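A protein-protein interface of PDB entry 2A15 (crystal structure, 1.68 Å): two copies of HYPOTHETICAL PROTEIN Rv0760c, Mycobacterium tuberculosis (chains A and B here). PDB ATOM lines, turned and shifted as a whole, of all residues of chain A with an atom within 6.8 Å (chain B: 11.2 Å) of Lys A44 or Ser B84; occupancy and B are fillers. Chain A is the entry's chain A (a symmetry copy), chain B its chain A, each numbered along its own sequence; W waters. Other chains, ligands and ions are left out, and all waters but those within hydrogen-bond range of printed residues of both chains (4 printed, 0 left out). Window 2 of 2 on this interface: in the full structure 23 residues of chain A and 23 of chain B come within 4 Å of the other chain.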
ATOM      1  N   PRO A  41      30.368 -10.523  -5.957  1.00  0.00           N
ATOM      2  CA  PRO A  41      30.708  -9.479  -4.975  1.00  0.00           C
ATOM      3  C   PRO A  41      30.927 -10.078  -3.604  1.00  0.00           C
ATOM      4  O   PRO A  41      30.755 -11.275  -3.407  1.00  0.00           O
ATOM      5  CB  PRO A  41      29.415  -8.644  -4.922  1.00  0.00           C
ATOM      6  CG  PRO A  41      28.299  -9.687  -5.098  1.00  0.00           C
ATOM      7  CD  PRO A  41      28.907 -10.781  -6.018  1.00  0.00           C
ATOM      8  N   ILE A  42      31.305  -9.218  -2.638  1.00  0.00           N
ATOM      9  CA  ILE A  42      31.311  -9.612  -1.239  1.00  0.00           C
ATOM     10  C   ILE A  42      29.839  -9.805  -0.795  1.00  0.00           C
ATOM     11  O   ILE A  42      28.979  -8.962  -1.106  1.00  0.00           O
ATOM     12  CB  ILE A  42      31.908  -8.477  -0.392  1.00  0.00           C
ATOM     13  CG1 ILE A  42      33.349  -8.204  -0.808  1.00  0.00           C
ATOM     14  CG2 ILE A  42      31.827  -8.844   1.093  1.00  0.00           C
ATOM     15  CD1 ILE A  42      33.849  -6.837  -0.280  1.00  0.00           C
ATOM     16  N   GLY A  43      29.578 -10.901  -0.096  1.00  0.00           N
ATOM     17  CA  GLY A  43      28.227 -11.239   0.380  1.00  0.00           C
ATOM     18  C   GLY A  43      27.487 -12.110  -0.626  1.00  0.00           C
ATOM     19  O   GLY A  43      27.913 -12.260  -1.779  1.00  0.00           O
ATOM     20  N   LYS A  44      26.326 -12.612  -0.206  1.00  0.00           N
ATOM     21  CA  LYS A  44      25.651 -13.656  -1.000  1.00  0.00           C
ATOM     22  C   LYS A  44      25.018 -13.056  -2.250  1.00  0.00           C
ATOM     23  O   LYS A  44      24.306 -12.026  -2.185  1.00  0.00           O
ATOM     24  CB  LYS A  44      24.585 -14.371  -0.134  1.00  0.00           C
ATOM     25  CG  LYS A  44      23.921 -15.553  -0.844  1.00  0.00           C
ATOM     26  CD  LYS A  44      22.997 -16.299   0.155  1.00  0.00           C
ATOM     27  CE  LYS A  44      22.352 -17.536  -0.457  1.00  0.00           C
ATOM     28  NZ  LYS A  44      21.333 -17.206  -1.503  1.00  0.00           N
ATOM     29  N   SER A  45      25.268 -13.697  -3.399  1.00  0.00           N
ATOM     30  CA  SER A  45      24.743 -13.255  -4.689  1.00  0.00           C
ATOM     31  C   SER A  45      24.877 -14.402  -5.672  1.00  0.00           C
ATOM     32  O   SER A  45      25.442 -15.456  -5.330  1.00  0.00           O
ATOM     33  CB  SER A  45      25.452 -12.004  -5.227  1.00  0.00           C
ATOM     34  OG  SER A  45      24.700 -11.316  -6.247  1.00  0.00           O
ATOM     35  N   VAL A  46      24.358 -14.191  -6.884  1.00  0.00           N
ATOM     36  CA  VAL A  46      24.406 -15.249  -7.924  1.00  0.00           C
ATOM     37  C   VAL A  46      25.856 -15.735  -8.150  1.00  0.00           C
ATOM     38  O   VAL A  46      26.114 -16.939  -8.265  1.00  0.00           O
ATOM     39  CB  VAL A  46      23.814 -14.751  -9.242  1.00  0.00           C
ATOM     40  CG1 VAL A  46      24.031 -15.799 -10.373  1.00  0.00           C
ATOM     41  CG2 VAL A  46      22.307 -14.444  -9.044  1.00  0.00           C
ATOM     42  N   THR A  47      26.784 -14.789  -8.168  1.00  0.00           N
ATOM     43  CA  THR A  47      28.207 -15.070  -8.431  1.00  0.00           C
ATOM     44  C   THR A  47      29.028 -15.337  -7.134  1.00  0.00           C
ATOM     45  O   THR A  47      30.252 -15.495  -7.206  1.00  0.00           O
ATOM     46  CB  THR A  47      28.821 -13.897  -9.218  1.00  0.00           C
ATOM     47  OG1 THR A  47      28.519 -12.676  -8.527  1.00  0.00           O
ATOM     48  CG2 THR A  47      28.189 -13.766 -10.623  1.00  0.00           C
ATOM     49  N   ASN A  48      28.346 -15.375  -5.977  1.00  0.00           N
ATOM     50  CA  ASN A  48      28.928 -15.741  -4.685  1.00  0.00           C
ATOM     51  C   ASN A  48      27.865 -16.463  -3.859  1.00  0.00           C
ATOM     52  O   ASN A  48      27.392 -15.968  -2.859  1.00  0.00           O
ATOM     53  CB  ASN A  48      29.488 -14.475  -3.973  1.00  0.00           C
ATOM     54  CG  ASN A  48      30.286 -14.803  -2.709  1.00  0.00           C
ATOM     55  OD1 ASN A  48      30.400 -15.950  -2.320  1.00  0.00           O
ATOM     56  ND2 ASN A  48      30.812 -13.765  -2.037  1.00  0.00           N
ATOM     57  N   PRO A  49      27.433 -17.658  -4.323  1.00  0.00           N
ATOM     58  CA  PRO A  49      26.181 -18.237  -3.838  1.00  0.00           C
ATOM     59  C   PRO A  49      26.117 -18.548  -2.347  1.00  0.00           C
ATOM     60  O   PRO A  49      25.024 -18.504  -1.767  1.00  0.00           O
ATOM     61  CB  PRO A  49      26.047 -19.517  -4.685  1.00  0.00           C
ATOM     62  CG  PRO A  49      26.862 -19.254  -5.908  1.00  0.00           C
ATOM     63  CD  PRO A  49      28.040 -18.486  -5.384  1.00  0.00           C
ATOM     64  N   ASP A  50      27.252 -18.840  -1.710  1.00  0.00           N
ATOM     65  CA  ASP A  50      27.217 -19.081  -0.274  1.00  0.00           C
ATOM     66  C   ASP A  50      27.610 -17.869   0.575  1.00  0.00           C
ATOM     67  O   ASP A  50      27.572 -17.927   1.805  1.00  0.00           O
ATOM     68  CB  ASP A  50      27.994 -20.352   0.134  1.00  0.00           C
ATOM     69  CG  ASP A  50      29.520 -20.170   0.170  1.00  0.00           C
ATOM     70  OD1 ASP A  50      30.063 -19.053  -0.006  1.00  0.00           O
ATOM     71  OD2 ASP A  50      30.199 -21.196   0.388  1.00  0.00           O
ATOM     72  N   GLY A  51      27.986 -16.781  -0.089  1.00  0.00           N
ATOM     73  CA  GLY A  51      28.349 -15.547   0.604  1.00  0.00           C
ATOM     74  C   GLY A  51      29.728 -15.479   1.222  1.00  0.00           C
ATOM     75  O   GLY A  51      30.063 -14.472   1.832  1.00  0.00           O
ATOM     76  N   SER A  52      30.514 -16.545   1.100  1.00  0.00           N
ATOM     77  CA  SER A  52      31.835 -16.536   1.716  1.00  0.00           C
ATOM     78  C   SER A  52      32.979 -16.576   0.691  1.00  0.00           C
ATOM     79  O   SER A  52      34.155 -16.707   1.068  1.00  0.00           O
ATOM     80  CB  SER A  52      31.945 -17.687   2.729  1.00  0.00           C
ATOM     81  OG  SER A  52      32.080 -18.917   2.056  1.00  0.00           O
ATOM     82  N   GLY A 126      34.599  -7.565  -4.599  1.00  0.00           N
ATOM     83  CA  GLY A 126      33.773  -6.549  -5.279  1.00  0.00           C
ATOM     84  C   GLY A 126      32.640  -5.953  -4.425  1.00  0.00           C
ATOM     85  O   GLY A 126      31.912  -6.694  -3.718  1.00  0.00           O
ATOM     86  N   TYR A 127      32.505  -4.628  -4.498  1.00  0.00           N
ATOM     87  CA  TYR A 127      31.458  -3.882  -3.773  1.00  0.00           C
ATOM     88  C   TYR A 127      30.378  -3.543  -4.772  1.00  0.00           C
ATOM     89  O   TYR A 127      30.367  -2.486  -5.408  1.00  0.00           O
ATOM     90  CB  TYR A 127      32.041  -2.613  -3.095  1.00  0.00           C
ATOM     91  CG  TYR A 127      32.984  -2.976  -2.002  1.00  0.00           C
ATOM     92  CD1 TYR A 127      32.560  -2.951  -0.638  1.00  0.00           C
ATOM     93  CD2 TYR A 127      34.354  -3.310  -2.287  1.00  0.00           C
ATOM     94  CE1 TYR A 127      33.445  -3.309   0.412  1.00  0.00           C
ATOM     95  CE2 TYR A 127      35.241  -3.642  -1.226  1.00  0.00           C
ATOM     96  CZ  TYR A 127      34.797  -3.662   0.098  1.00  0.00           C
ATOM     97  OH  TYR A 127      35.698  -4.005   1.094  1.00  0.00           O
ATOM     98  N   TRP A 128      29.454  -4.512  -4.921  1.00  0.00           N
ATOM     99  CA  TRP A 128      28.227  -4.276  -5.679  1.00  0.00           C
ATOM    100  C   TRP A 128      27.178  -5.310  -5.279  1.00  0.00           C
ATOM    101  O   TRP A 128      27.454  -6.260  -4.547  1.00  0.00           O
ATOM    102  CB  TRP A 128      28.465  -4.322  -7.198  1.00  0.00           C
ATOM    103  CG  TRP A 128      28.980  -5.672  -7.705  1.00  0.00           C
ATOM    104  CD1 TRP A 128      30.287  -6.098  -7.717  1.00  0.00           C
ATOM    105  CD2 TRP A 128      28.204  -6.741  -8.292  1.00  0.00           C
ATOM    106  NE1 TRP A 128      30.366  -7.379  -8.246  1.00  0.00           N
ATOM    107  CE2 TRP A 128      29.107  -7.783  -8.623  1.00  0.00           C
ATOM    108  CE3 TRP A 128      26.831  -6.918  -8.567  1.00  0.00           C
ATOM    109  CZ2 TRP A 128      28.681  -9.000  -9.216  1.00  0.00           C
ATOM    110  CZ3 TRP A 128      26.418  -8.114  -9.165  1.00  0.00           C
ATOM    111  CH2 TRP A 128      27.336  -9.132  -9.483  1.00  0.00           C
ATOM    112  N   ASN A 129      25.957  -5.073  -5.770  1.00  0.00           N
ATOM    113  CA  ASN A 129      24.862  -6.027  -5.550  1.00  0.00           C
ATOM    114  C   ASN A 129      23.886  -5.958  -6.729  1.00  0.00           C
ATOM    115  O   ASN A 129      23.979  -5.064  -7.601  1.00  0.00           O
ATOM    116  CB  ASN A 129      24.217  -5.784  -4.178  1.00  0.00           C
ATOM    117  CG  ASN A 129      23.522  -4.417  -4.078  1.00  0.00           C
ATOM    118  OD1 ASN A 129      22.739  -4.028  -4.960  1.00  0.00           O
ATOM    119  ND2 ASN A 129      23.828  -3.683  -3.022  1.00  0.00           N
ATOM    120  N   LEU A 130      22.988  -6.967  -6.769  1.00  0.00           N
ATOM    121  CA  LEU A 130      22.093  -7.103  -7.895  1.00  0.00           C
ATOM    122  C   LEU A 130      21.229  -5.852  -8.073  1.00  0.00           C
ATOM    123  O   LEU A 130      20.894  -5.479  -9.223  1.00  0.00           O
ATOM    124  CB  LEU A 130      21.243  -8.359  -7.694  1.00  0.00           C
ATOM    125  CG  LEU A 130      21.991  -9.709  -7.755  1.00  0.00           C
ATOM    126  CD1 LEU A 130      21.147 -10.848  -7.089  1.00  0.00           C
ATOM    127  CD2 LEU A 130      22.277 -10.016  -9.210  1.00  0.00           C
ATOM    128  N   SER B   7      21.901  -0.091   5.980  1.00  0.00           N
ATOM    129  CA  SER B   7      22.653  -1.229   6.436  1.00  0.00           C
ATOM    130  C   SER B   7      23.538  -0.832   7.643  1.00  0.00           C
ATOM    131  O   SER B   7      23.870   0.347   7.772  1.00  0.00           O
ATOM    132  CB  SER B   7      23.550  -1.789   5.323  1.00  0.00           C
ATOM    133  OG  SER B   7      24.821  -1.161   5.410  1.00  0.00           O
ATOM    134  N   PRO B   8      23.935  -1.801   8.486  1.00  0.00           N
ATOM    135  CA  PRO B   8      24.851  -1.511   9.587  1.00  0.00           C
ATOM    136  C   PRO B   8      26.160  -0.897   9.071  1.00  0.00           C
ATOM    137  O   PRO B   8      26.716  -0.011   9.707  1.00  0.00           O
ATOM    138  CB  PRO B   8      25.156  -2.892  10.165  1.00  0.00           C
ATOM    139  CG  PRO B   8      23.933  -3.715   9.832  1.00  0.00           C
ATOM    140  CD  PRO B   8      23.508  -3.221   8.501  1.00  0.00           C
ATOM    141  N   ALA B   9      26.648  -1.376   7.933  1.00  0.00           N
ATOM    142  CA  ALA B   9      27.875  -0.739   7.366  1.00  0.00           C
ATOM    143  C   ALA B   9      27.702   0.700   6.951  1.00  0.00           C
ATOM    144  O   ALA B   9      28.634   1.527   7.182  1.00  0.00           O
ATOM    145  CB  ALA B   9      28.490  -1.610   6.213  1.00  0.00           C
ATOM    146  N   LEU B  10      26.552   1.048   6.331  1.00  0.00           N
ATOM    147  CA  LEU B  10      26.316   2.373   5.891  1.00  0.00           C
ATOM    148  C   LEU B  10      26.142   3.259   7.136  1.00  0.00           C
ATOM    149  O   LEU B  10      26.681   4.349   7.198  1.00  0.00           O
ATOM    150  CB  LEU B  10      25.072   2.461   5.029  1.00  0.00           C
ATOM    151  CG  LEU B  10      24.783   3.861   4.497  1.00  0.00           C
ATOM    152  CD1 LEU B  10      25.932   4.486   3.702  1.00  0.00           C
ATOM    153  CD2 LEU B  10      23.464   3.879   3.682  1.00  0.00           C
ATOM    154  N   THR B  80      29.118   6.155  -3.020  1.00  0.00           N
ATOM    155  CA  THR B  80      29.010   5.026  -2.115  1.00  0.00           C
ATOM    156  C   THR B  80      28.729   3.773  -2.926  1.00  0.00           C
ATOM    157  O   THR B  80      27.912   3.809  -3.860  1.00  0.00           O
ATOM    158  CB  THR B  80      27.862   5.232  -1.083  1.00  0.00           C
ATOM    159  OG1 THR B  80      28.231   6.288  -0.162  1.00  0.00           O
ATOM    160  CG2 THR B  80      27.560   3.957  -0.301  1.00  0.00           C
ATOM    161  N   PHE B  81      29.416   2.695  -2.548  1.00  0.00           N
ATOM    162  CA  PHE B  81      29.304   1.384  -3.195  1.00  0.00           C
ATOM    163  C   PHE B  81      28.975   0.301  -2.157  1.00  0.00           C
ATOM    164  O   PHE B  81      29.828  -0.311  -1.526  1.00  0.00           O
ATOM    165  CB  PHE B  81      30.613   1.030  -3.921  1.00  0.00           C
ATOM    166  CG  PHE B  81      30.932   1.956  -5.063  1.00  0.00           C
ATOM    167  CD1 PHE B  81      30.458   1.684  -6.340  1.00  0.00           C
ATOM    168  CD2 PHE B  81      31.694   3.120  -4.854  1.00  0.00           C
ATOM    169  CE1 PHE B  81      30.756   2.511  -7.413  1.00  0.00           C
ATOM    170  CE2 PHE B  81      32.012   3.953  -5.935  1.00  0.00           C
ATOM    171  CZ  PHE B  81      31.544   3.637  -7.209  1.00  0.00           C
ATOM    172  N   PRO B  82      27.658   0.042  -1.971  1.00  0.00           N
ATOM    173  CA  PRO B  82      27.226  -1.066  -1.175  1.00  0.00           C
ATOM    174  C   PRO B  82      27.800  -2.378  -1.750  1.00  0.00           C
ATOM    175  O   PRO B  82      28.068  -2.441  -2.989  1.00  0.00           O
ATOM    176  CB  PRO B  82      25.696  -1.052  -1.403  1.00  0.00           C
ATOM    177  CG  PRO B  82      25.373   0.314  -1.747  1.00  0.00           C
ATOM    178  CD  PRO B  82      26.532   0.782  -2.574  1.00  0.00           C
ATOM    179  N   SER B  83      27.998  -3.388  -0.900  1.00  0.00           N
ATOM    180  CA  SER B  83      28.289  -4.737  -1.426  1.00  0.00           C
ATOM    181  C   SER B  83      27.008  -5.567  -1.321  1.00  0.00           C
ATOM    182  O   SER B  83      25.926  -4.990  -1.189  1.00  0.00           O
ATOM    183  CB  SER B  83      29.417  -5.406  -0.635  1.00  0.00           C
ATOM    184  OG  SER B  83      29.009  -5.736   0.678  1.00  0.00           O
ATOM    185  N   SER B  84      27.159  -6.880  -1.357  1.00  0.00           N
ATOM    186  CA  SER B  84      25.991  -7.776  -1.124  1.00  0.00           C
ATOM    187  C   SER B  84      25.925  -8.262   0.312  1.00  0.00           C
ATOM    188  O   SER B  84      25.123  -9.150   0.674  1.00  0.00           O
ATOM    189  CB  SER B  84      25.994  -8.950  -2.115  1.00  0.00           C
ATOM    190  OG  SER B  84      25.819  -8.434  -3.415  1.00  0.00           O
ATOM    191  N   SER B  85      26.802  -7.700   1.138  1.00  0.00           N
ATOM    192  CA  SER B  85      26.817  -7.968   2.564  1.00  0.00           C
ATOM    193  C   SER B  85      26.405  -6.682   3.287  1.00  0.00           C
ATOM    194  O   SER B  85      26.983  -5.626   3.051  1.00  0.00           O
ATOM    195  CB  SER B  85      28.230  -8.320   3.044  1.00  0.00           C
ATOM    196  OG  SER B  85      28.249  -8.375   4.473  1.00  0.00           O
ATOM    197  N   PRO B  86      25.424  -6.754   4.206  1.00  0.00           N
ATOM    198  CA  PRO B  86      25.071  -5.546   4.994  1.00  0.00           C
ATOM    199  C   PRO B  86      26.207  -5.043   5.916  1.00  0.00           C
ATOM    200  O   PRO B  86      26.077  -3.960   6.499  1.00  0.00           O
ATOM    201  CB  PRO B  86      23.906  -6.055   5.892  1.00  0.00           C
ATOM    202  CG  PRO B  86      23.310  -7.198   5.051  1.00  0.00           C
ATOM    203  CD  PRO B  86      24.550  -7.900   4.559  1.00  0.00           C
ATOM    204  N   ASP B  87      27.266  -5.834   6.051  1.00  0.00           N
ATOM    205  CA  ASP B  87      28.364  -5.506   6.961  1.00  0.00           C
ATOM    206  C   ASP B  87      29.638  -5.003   6.307  1.00  0.00           C
ATOM    207  O   ASP B  87      30.604  -4.730   7.010  1.00  0.00           O
ATOM    208  CB  ASP B  87      28.689  -6.694   7.850  1.00  0.00           C
ATOM    209  CG  ASP B  87      27.490  -7.078   8.798  1.00  0.00           C
ATOM    210  OD1 ASP B  87      26.522  -6.294   8.899  1.00  0.00           O
ATOM    211  OD2 ASP B  87      27.557  -8.163   9.376  1.00  0.00           O
ATOM    212  N   GLU B  88      29.615  -4.867   4.987  1.00  0.00           N
ATOM    213  CA  GLU B  88      30.793  -4.311   4.242  1.00  0.00           C
ATOM    214  C   GLU B  88      30.360  -3.331   3.196  1.00  0.00           C
ATOM    215  O   GLU B  88      29.386  -3.558   2.450  1.00  0.00           O
ATOM    216  CB  GLU B  88      31.646  -5.431   3.628  1.00  0.00           C
ATOM    217  CG  GLU B  88      32.178  -6.426   4.647  1.00  0.00           C
ATOM    218  CD  GLU B  88      33.387  -7.200   4.194  1.00  0.00           C
ATOM    219  OE1 GLU B  88      34.412  -6.598   3.803  1.00  0.00           O
ATOM    220  OE2 GLU B  88      33.334  -8.445   4.278  1.00  0.00           O
ATOM    221  N   ILE B  89      31.091  -2.217   3.115  1.00  0.00           N
ATOM    222  CA  ILE B  89      30.764  -1.163   2.205  1.00  0.00           C
ATOM    223  C   ILE B  89      32.069  -0.417   1.791  1.00  0.00           C
ATOM    224  O   ILE B  89      33.058  -0.458   2.515  1.00  0.00           O
ATOM    225  CB  ILE B  89      29.711  -0.170   2.843  1.00  0.00           C
ATOM    226  CG1 ILE B  89      29.113   0.773   1.795  1.00  0.00           C
ATOM    227  CG2 ILE B  89      30.388   0.650   3.970  1.00  0.00           C
ATOM    228  CD1 ILE B  89      27.817   1.476   2.318  1.00  0.00           C
ATOM    229  N   ALA B  90      32.016   0.208   0.617  1.00  0.00           N
ATOM    230  CA  ALA B  90      33.130   1.076   0.146  1.00  0.00           C
ATOM    231  C   ALA B  90      32.608   2.459  -0.257  1.00  0.00           C
ATOM    232  O   ALA B  90      31.457   2.602  -0.669  1.00  0.00           O
ATOM    233  CB  ALA B  90      33.823   0.402  -1.045  1.00  0.00           C
ATOM    234  N   TYR B 113      34.960  -0.313   4.570  1.00  0.00           N
ATOM    235  CA  TYR B 113      34.618  -0.491   5.980  1.00  0.00           C
ATOM    236  C   TYR B 113      34.021  -1.879   6.179  1.00  0.00           C
ATOM    237  O   TYR B 113      33.264  -2.353   5.335  1.00  0.00           O
ATOM    238  CB  TYR B 113      33.552   0.510   6.448  1.00  0.00           C
ATOM    239  CG  TYR B 113      33.960   1.977   6.388  1.00  0.00           C
ATOM    240  CD1 TYR B 113      34.123   2.729   7.567  1.00  0.00           C
ATOM    241  CD2 TYR B 113      34.149   2.613   5.164  1.00  0.00           C
ATOM    242  CE1 TYR B 113      34.481   4.070   7.501  1.00  0.00           C
ATOM    243  CE2 TYR B 113      34.526   3.953   5.097  1.00  0.00           C
ATOM    244  CZ  TYR B 113      34.669   4.674   6.275  1.00  0.00           C
ATOM    245  OH  TYR B 113      35.026   6.002   6.200  1.00  0.00           O
ATOM    246  N   LYS B 117      28.725  -8.132  13.698  1.00  0.00           N
ATOM    247  CA  LYS B 117      27.259  -8.320  13.802  1.00  0.00           C
ATOM    248  C   LYS B 117      26.561  -7.321  14.724  1.00  0.00           C
ATOM    249  O   LYS B 117      25.399  -6.913  14.476  1.00  0.00           O
ATOM    250  CB  LYS B 117      26.916  -9.762  14.193  1.00  0.00           C
ATOM    251  CG  LYS B 117      27.106 -10.759  13.049  1.00  0.00           C
ATOM    252  CD  LYS B 117      26.448 -10.290  11.736  1.00  0.00           C
ATOM    253  CE  LYS B 117      26.657 -11.310  10.615  1.00  0.00           C
ATOM    254  NZ  LYS B 117      25.807 -10.981   9.428  1.00  0.00           N
HETATM  255  O   HOH W   1      23.671  -9.196  -4.904  1.00  0.00           O
HETATM  256  O   HOH W   2      25.384 -11.598   2.563  1.00  0.00           O
HETATM  257  O   HOH W   3      34.972  -3.993   3.606  1.00  0.00           O
HETATM  258  O   HOH W   4      23.133 -10.505  -0.514  1.00  0.00           O
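N of Ser B84 sits at hydrogen-bond distance from O of Ile A42, at 2.8 Å. The backbone NH of Ser B85 sits at hydrogen-bond distance from the backbone carbonyl oxygen of Ile A42, 3.4 Å away. The backbone carbonyl oxygen (O) of Ser B83 is in hydrogen-bond range of the side-chain amide nitrogen (ND2) of Asn A129 (3.1 Å). O of Tyr A127 sits close to O of Pro B82, 3.3 Å away. The backbone carbonyl oxygen (O) of Pro B82 is in hydrogen-bond range of the backbone NH (N) of Trp A128 (3.2 Å). OG of Ser B84 sits at hydrogen-bond distance from O of Trp A128 (2.9 Å).
The backbone carbonyl oxygen of Gly A43 sits at hydrogen-bond distance from the side-chain amide nitrogen of Asn A48. The side-chain hydroxyl (OG) of Ser B83 lies within hydrogen-bond range of the backbone carbonyl oxygen (O) of Glu B88 (2.8 Å). The backbone carbonyl oxygen of Ile B89 sits at hydrogen-bond distance from the backbone NH of Tyr B113, 2.8 Å away. The backbone carbonyl oxygen (O) of Gly A126 lies within hydrogen-bond range of the backbone NH (N) of Ile A42. ND2 of Asn A48 is in hydrogen-bond range of O of Pro A41, at 2.8 Å. The side-chain hydroxyl of Ser B83 is in hydrogen-bond range of the backbone NH of Ser B85 (3.0 Å).
Among the printed residues, pairs that only touch across the chains: Asn A129 with Ser B84, Pro A41 with Ser B84, Trp A128 with Ser B83, Tyr A127 with Ala B90, Tyr A127 with Ile B89, Lys A44 with Ser B84, Ile A42 with Glu B88, Tyr A127 with Phe B81, Asn A129 with Pro B82, Ile A42 with Ser B83, Gly A43 with Ser B84, Gly A43 with Ser B85, Tyr A127 with Glu B88 and Tyr A127 with Ser B83.
Of chain B, only Ser B84 comes within 4 Å of Pro A41. Of chain B, only Ser B83, Ser B84, Ser B85 and Glu B88 come within 4 Å of Ile A42. Printed residues of chain B within 4 Å of Gly A43: Ser B84 (3.8 Å) and Ser B85 (3.9 Å). Lys A44 touches just one residue of chain B: Ser B84. No residue of chain B comes within 4 Å of Ser A45. No residue of chain B comes within 4 Å of Asn A48. Gly A126 touches none of the printed residues of chain B. Of chain B, only Pro B82 (3.2 Å), Ser B83 (3.3 Å) and Ser B84 (2.9 Å) come within 4 Å of Trp A128. Asn A129 touches three residues of chain B. Of the printed residues of chain A, Phe B81 touches Tyr A127 (3.6 Å). Of the printed residues of chain A, Pro B82 touches Tyr A127 (3.1 Å), Trp A128 (3.2 Å) and Asn A129 (3.6 Å). Ser B84 touches six residues of chain A. The nearest residue of chain B that does not touch Lys A44 is Ser B85 (5.1 Å). The nearest residue of chain A that does not touch Ser B84 is Ser A45 (4.02 Å).
Of the 17 printed residues of chain B, 8 touch a printed residue of chain A. Along chain B the printed residues that touch a printed residue of chain A span positions 81 to 90. Of the 17 printed residues of chain A, 7 touch a printed residue of chain B. Printed residues of chain A that touch a printed residue of chain B: Pro A41, Ile A42, Gly A43, Lys A44, Tyr A127, Trp A128 and Asn A129. Hydrophobic or aromatic side chains of chain A that line the printed part of chain B: Pro A41, Ile A42 and Tyr A127. Among the printed residues, 20 pairs touch across the chains. Among the printed residues, no Asp or Glu carboxylate lies within 4 Å of a Lys or Arg side-chain nitrogen of the other chain.
No position is printed for both chains. Of the 20 pairs that touch across the chains among the printed residues, none has its exchanged pair printed and touching as well.
Water W4 lies within hydrogen-bond range of the backbone carbonyl oxygen of Lys A44 (2.5 Å) and the backbone carbonyl oxygen of Ser B84 (2.7 Å). Water W3 lies within hydrogen-bond range of OH of Tyr A127 (2.6 Å), OE1 of Glu B88 (2.7 Å) and O of Tyr B113 (2.9 Å). Water W1 lies within hydrogen-bond range of OG of Ser A45, OG of Ser B84 and N of Leu A130. Water W2 lies within hydrogen-bond range of the backbone NH of Lys A44 (3.1 Å) and the backbone carbonyl oxygen of Ser B84 (3.1 Å).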
